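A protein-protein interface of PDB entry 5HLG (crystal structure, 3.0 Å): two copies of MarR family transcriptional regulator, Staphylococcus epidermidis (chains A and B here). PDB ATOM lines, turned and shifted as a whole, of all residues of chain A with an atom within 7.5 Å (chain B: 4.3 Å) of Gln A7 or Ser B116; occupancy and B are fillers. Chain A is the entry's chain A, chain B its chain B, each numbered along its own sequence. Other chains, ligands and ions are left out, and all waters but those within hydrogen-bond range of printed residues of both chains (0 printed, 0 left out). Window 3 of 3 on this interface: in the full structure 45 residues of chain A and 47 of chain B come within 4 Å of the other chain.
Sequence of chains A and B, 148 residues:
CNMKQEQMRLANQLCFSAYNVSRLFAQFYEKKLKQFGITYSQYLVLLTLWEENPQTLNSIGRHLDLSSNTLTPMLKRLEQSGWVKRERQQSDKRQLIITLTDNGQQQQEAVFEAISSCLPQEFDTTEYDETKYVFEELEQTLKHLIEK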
ATOM      1  N   GLN A   5      -1.347   6.778  22.550  1.00  0.00           N
ATOM      2  CA  GLN A   5      -1.659   8.176  22.946  1.00  0.00           C
ATOM      3  C   GLN A   5      -3.049   8.597  22.494  1.00  0.00           C
ATOM      4  O   GLN A   5      -3.809   9.189  23.263  1.00  0.00           O
ATOM      5  CB  GLN A   5      -0.619   9.149  22.377  1.00  0.00           C
ATOM      6  CG  GLN A   5      -0.974  10.642  22.602  1.00  0.00           C
ATOM      7  CD  GLN A   5       0.171  11.450  23.184  1.00  0.00           C
ATOM      8  OE1 GLN A   5       1.331  11.223  22.849  1.00  0.00           O
ATOM      9  NE2 GLN A   5      -0.153  12.409  24.060  1.00  0.00           N
ATOM     10  N   GLU A   6      -3.372   8.307  21.241  1.00  0.00           N
ATOM     11  CA  GLU A   6      -4.678   8.690  20.689  1.00  0.00           C
ATOM     12  C   GLU A   6      -5.857   7.876  21.254  1.00  0.00           C
ATOM     13  O   GLU A   6      -7.009   8.312  21.176  1.00  0.00           O
ATOM     14  CB  GLU A   6      -4.705   8.569  19.159  1.00  0.00           C
ATOM     15  CG  GLU A   6      -3.856   9.658  18.399  1.00  0.00           C
ATOM     16  CD  GLU A   6      -4.615  10.958  18.247  1.00  0.00           C
ATOM     17  OE1 GLU A   6      -5.854  10.909  18.111  1.00  0.00           O
ATOM     18  OE2 GLU A   6      -3.969  12.026  18.252  1.00  0.00           O
ATOM     19  N   GLN A   7      -5.578   6.674  21.757  1.00  0.00           N
ATOM     20  CA  GLN A   7      -6.589   5.866  22.449  1.00  0.00           C
ATOM     21  C   GLN A   7      -6.944   6.441  23.834  1.00  0.00           C
ATOM     22  O   GLN A   7      -8.036   6.191  24.347  1.00  0.00           O
ATOM     23  CB  GLN A   7      -6.176   4.368  22.554  1.00  0.00           C
ATOM     24  CG  GLN A   7      -4.917   4.065  23.361  1.00  0.00           C
ATOM     25  CD  GLN A   7      -4.858   2.615  23.844  1.00  0.00           C
ATOM     26  OE1 GLN A   7      -5.255   1.696  23.127  1.00  0.00           O
ATOM     27  NE2 GLN A   7      -4.362   2.403  25.066  1.00  0.00           N
ATOM     28  N   MET A   8      -6.016   7.181  24.444  1.00  0.00           N
ATOM     29  CA  MET A   8      -6.297   7.887  25.696  1.00  0.00           C
ATOM     30  C   MET A   8      -7.120   9.130  25.411  1.00  0.00           C
ATOM     31  O   MET A   8      -8.055   9.443  26.156  1.00  0.00           O
ATOM     32  CB  MET A   8      -4.999   8.295  26.407  1.00  0.00           C
ATOM     33  CG  MET A   8      -4.523   7.292  27.438  1.00  0.00           C
ATOM     34  SD  MET A   8      -5.588   7.230  28.905  1.00  0.00           S
ATOM     35  CE  MET A   8      -5.196   8.803  29.643  1.00  0.00           C
ATOM     36  N   ARG A   9      -6.759   9.838  24.342  1.00  0.00           N
ATOM     37  CA  ARG A   9      -7.467  11.042  23.945  1.00  0.00           C
ATOM     38  C   ARG A   9      -8.947  10.735  23.705  1.00  0.00           C
ATOM     39  O   ARG A   9      -9.806  11.541  24.031  1.00  0.00           O
ATOM     40  CB  ARG A   9      -6.807  11.661  22.717  1.00  0.00           C
ATOM     41  CG  ARG A   9      -7.450  12.939  22.246  1.00  0.00           C
ATOM     42  CD  ARG A   9      -6.728  13.508  21.042  1.00  0.00           C
ATOM     43  NE  ARG A   9      -7.318  14.762  20.538  1.00  0.00           N
ATOM     44  CZ  ARG A   9      -8.324  14.901  19.673  1.00  0.00           C
ATOM     45  NH1 ARG A   9      -8.920  13.858  19.097  1.00  0.00           N
ATOM     46  NH2 ARG A   9      -8.736  16.131  19.367  1.00  0.00           N
ATOM     47  N   LEU A  10      -9.230   9.560  23.159  1.00  0.00           N
ATOM     48  CA  LEU A  10     -10.590   9.099  22.981  1.00  0.00           C
ATOM     49  C   LEU A  10     -11.317   8.791  24.273  1.00  0.00           C
ATOM     50  O   LEU A  10     -12.457   9.212  24.460  1.00  0.00           O
ATOM     51  CB  LEU A  10     -10.545   7.814  22.162  1.00  0.00           C
ATOM     52  CG  LEU A  10     -11.857   7.438  21.495  1.00  0.00           C
ATOM     53  CD1 LEU A  10     -12.195   8.379  20.344  1.00  0.00           C
ATOM     54  CD2 LEU A  10     -11.805   5.998  21.033  1.00  0.00           C
ATOM     55  N   ALA A  11     -10.661   8.040  25.153  1.00  0.00           N
ATOM     56  CA  ALA A  11     -11.285   7.596  26.397  1.00  0.00           C
ATOM     57  C   ALA A  11     -11.643   8.786  27.268  1.00  0.00           C
ATOM     58  O   ALA A  11     -12.680   8.779  27.919  1.00  0.00           O
ATOM     59  CB  ALA A  11     -10.368   6.638  27.144  1.00  0.00           C
ATOM     60  N   ASN A  12     -10.809   9.825  27.223  1.00  0.00           N
ATOM     61  CA  ASN A  12     -11.026  11.027  28.015  1.00  0.00           C
ATOM     62  C   ASN A  12     -12.212  11.866  27.530  1.00  0.00           C
ATOM     63  O   ASN A  12     -13.065  12.265  28.317  1.00  0.00           O
ATOM     64  CB  ASN A  12      -9.758  11.889  28.028  1.00  0.00           C
ATOM     65  CG  ASN A  12      -8.706  11.365  28.978  1.00  0.00           C
ATOM     66  OD1 ASN A  12      -8.950  10.429  29.754  1.00  0.00           O
ATOM     67  ND2 ASN A  12      -7.522  11.980  28.935  1.00  0.00           N
ATOM     68  N   PHE B 112      -1.331   9.033  32.687  1.00  0.00           N
ATOM     69  CA  PHE B 112      -1.871   8.598  31.403  1.00  0.00           C
ATOM     70  C   PHE B 112      -1.530   7.132  31.151  1.00  0.00           C
ATOM     71  O   PHE B 112      -2.401   6.345  30.769  1.00  0.00           O
ATOM     72  CB  PHE B 112      -1.378   9.495  30.261  1.00  0.00           C
ATOM     73  CG  PHE B 112      -2.248  10.707  30.013  1.00  0.00           C
ATOM     74  CD1 PHE B 112      -2.604  11.558  31.050  1.00  0.00           C
ATOM     75  CD2 PHE B 112      -2.702  11.001  28.734  1.00  0.00           C
ATOM     76  CE1 PHE B 112      -3.398  12.668  30.819  1.00  0.00           C
ATOM     77  CE2 PHE B 112      -3.496  12.111  28.498  1.00  0.00           C
ATOM     78  CZ  PHE B 112      -3.842  12.946  29.540  1.00  0.00           C
ATOM     79  N   GLU B 113      -0.282   6.757  31.431  1.00  0.00           N
ATOM     80  CA  GLU B 113       0.179   5.376  31.199  1.00  0.00           C
ATOM     81  C   GLU B 113      -0.611   4.399  32.085  1.00  0.00           C
ATOM     82  O   GLU B 113      -1.032   3.334  31.638  1.00  0.00           O
ATOM     83  CB  GLU B 113       1.697   5.232  31.437  1.00  0.00           C
ATOM     84  CG  GLU B 113       2.456   4.273  30.465  1.00  0.00           C
ATOM     85  CD  GLU B 113       2.104   2.808  30.657  1.00  0.00           C
ATOM     86  OE1 GLU B 113       2.498   2.219  31.685  1.00  0.00           O
ATOM     87  OE2 GLU B 113       1.452   2.237  29.754  1.00  0.00           O
ATOM     88  N   ALA B 114      -0.828   4.787  33.336  1.00  0.00           N
ATOM     89  CA  ALA B 114      -1.570   3.960  34.289  1.00  0.00           C
ATOM     90  C   ALA B 114      -2.986   3.632  33.821  1.00  0.00           C
ATOM     91  O   ALA B 114      -3.534   2.587  34.160  1.00  0.00           O
ATOM     92  CB  ALA B 114      -1.639   4.656  35.634  1.00  0.00           C
ATOM     93  N   ILE B 115      -3.592   4.549  33.080  1.00  0.00           N
ATOM     94  CA  ILE B 115      -4.933   4.342  32.538  1.00  0.00           C
ATOM     95  C   ILE B 115      -4.885   3.654  31.181  1.00  0.00           C
ATOM     96  O   ILE B 115      -5.675   2.733  30.929  1.00  0.00           O
ATOM     97  CB  ILE B 115      -5.699   5.674  32.391  1.00  0.00           C
ATOM     98  CG1 ILE B 115      -5.806   6.379  33.744  1.00  0.00           C
ATOM     99  CG2 ILE B 115      -7.097   5.435  31.824  1.00  0.00           C
ATOM    100  CD1 ILE B 115      -6.134   7.850  33.639  1.00  0.00           C
ATOM    101  N   SER B 116      -3.978   4.111  30.312  1.00  0.00           N
ATOM    102  CA  SER B 116      -3.889   3.606  28.930  1.00  0.00           C
ATOM    103  C   SER B 116      -3.525   2.135  28.847  1.00  0.00           C
ATOM    104  O   SER B 116      -4.043   1.403  28.004  1.00  0.00           O
ATOM    105  CB  SER B 116      -2.878   4.409  28.142  1.00  0.00           C
ATOM    106  OG  SER B 116      -2.704   3.908  26.824  1.00  0.00           O
ATOM    107  N   SER B 117      -2.630   1.710  29.726  1.00  0.00           N
ATOM    108  CA  SER B 117      -2.245   0.302  29.805  1.00  0.00           C
ATOM    109  C   SER B 117      -3.423  -0.657  30.071  1.00  0.00           C
ATOM    110  O   SER B 117      -3.335  -1.837  29.729  1.00  0.00           O
ATOM    111  CB  SER B 117      -1.156   0.107  30.864  1.00  0.00           C
ATOM    112  OG  SER B 117      -1.707   0.182  32.163  1.00  0.00           O
ATOM    113  N   CYS B 118      -4.515  -0.164  30.660  1.00  0.00           N
ATOM    114  CA  CYS B 118      -5.679  -1.007  30.956  1.00  0.00           C
ATOM    115  C   CYS B 118      -6.822  -0.882  29.938  1.00  0.00           C
ATOM    116  O   CYS B 118      -7.857  -1.541  30.089  1.00  0.00           O
ATOM    117  CB  CYS B 118      -6.210  -0.704  32.358  1.00  0.00           C
ATOM    118  SG  CYS B 118      -5.054  -1.101  33.690  1.00  0.00           S
ATOM    119  N   LEU B 119      -6.658  -0.036  28.920  1.00  0.00           N
ATOM    120  CA  LEU B 119      -7.661   0.071  27.853  1.00  0.00           C
ATOM    121  C   LEU B 119      -7.553  -1.060  26.836  1.00  0.00           C
ATOM    122  O   LEU B 119      -6.459  -1.349  26.343  1.00  0.00           O
ATOM    123  CB  LEU B 119      -7.560   1.402  27.118  1.00  0.00           C
ATOM    124  CG  LEU B 119      -7.886   2.642  27.960  1.00  0.00           C
ATOM    125  CD1 LEU B 119      -7.362   3.931  27.343  1.00  0.00           C
ATOM    126  CD2 LEU B 119      -9.390   2.733  28.172  1.00  0.00           C
ATOM    127  N   PHE B 123     -10.108  -0.139  20.974  1.00  0.00           N
ATOM    128  CA  PHE B 123      -9.988   1.256  20.566  1.00  0.00           C
ATOM    129  C   PHE B 123      -9.257   1.381  19.234  1.00  0.00           C
ATOM    130  O   PHE B 123      -8.027   1.341  19.183  1.00  0.00           O
ATOM    131  CB  PHE B 123      -9.263   2.066  21.642  1.00  0.00           C
ATOM    132  CG  PHE B 123     -10.142   2.479  22.788  1.00  0.00           C
ATOM    133  CD1 PHE B 123     -10.895   1.538  23.472  1.00  0.00           C
ATOM    134  CD2 PHE B 123     -10.217   3.805  23.179  1.00  0.00           C
ATOM    135  CE1 PHE B 123     -11.706   1.914  24.527  1.00  0.00           C
ATOM    136  CE2 PHE B 123     -11.026   4.187  24.233  1.00  0.00           C
ATOM    137  CZ  PHE B 123     -11.772   3.240  24.908  1.00  0.00           C
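Among the printed residues, pairs that only touch across the chains: Gln A7 with Phe B123, Leu A10 with Phe B123, Met A8 with Ile B115, Gln A7 with Leu B119, Asn A12 with Phe B112 and Ala A11 with Phe B123.
NE2 of Gln A7 is in hydrogen-bond range of OG of Ser B116.
SD of Met A8 is in hydrogen-bond range of N of Ser B116.
The backbone carbonyl oxygen (O) of Phe B112 lies close to the side-chain sulfur (SD) of Met A8 (3.8 Å).
Gln A7 touches three residues of chain B.
Of the printed residues of chain B, Met A8 touches Phe B112 (3.4 Å), Ile B115 (3.7 Å) and Ser B116 (3.4 Å).
Of the printed residues of chain B, Leu A10 touches Phe B123.
Of the printed residues of chain B, Ala A11 touches Phe B123 (3.9 Å).
Printed residues of chain A within 4 Å of Phe B112: Met A8 (3.4 Å) and Asn A12 (3.9 Å).
Ser B116 touches just these residues of chain A: Gln A7 (2.8 Å) and Met A8 (3.4 Å).
Of the printed residues of chain A, Phe B123 touches Gln A7 (3.4 Å), Leu A10 (3.5 Å) and Ala A11 (3.9 Å).
The nearest printed residue of chain B that does not touch Gln A7 is Ser B117 (5.0 Å).
Of the 9 printed residues of chain B, 5 touch a printed residue of chain A.
Hydrophobic or aromatic side chains of chain B that line the printed part of chain A: Phe B112, Ile B115, Leu B119 and Phe B123.
Printed residues of chain A that touch a printed residue of chain B: Gln A7, Met A8, Leu A10, Ala A11 and Asn A12.
Hydrophobic or aromatic side chains of chain A within 4 Å of the printed part of chain B: Met A8, Leu A10 and Ala A11.
Among the printed residues, 9 pairs touch across the chains.
Among the printed residues, no Asp or Glu carboxylate lies within 4 Å of a Lys or Arg side-chain nitrogen of the other chain.
No position is printed for both chains.
Of the 9 pairs that touch across the chains among the printed residues, none has its exchanged pair printed and touching as well.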
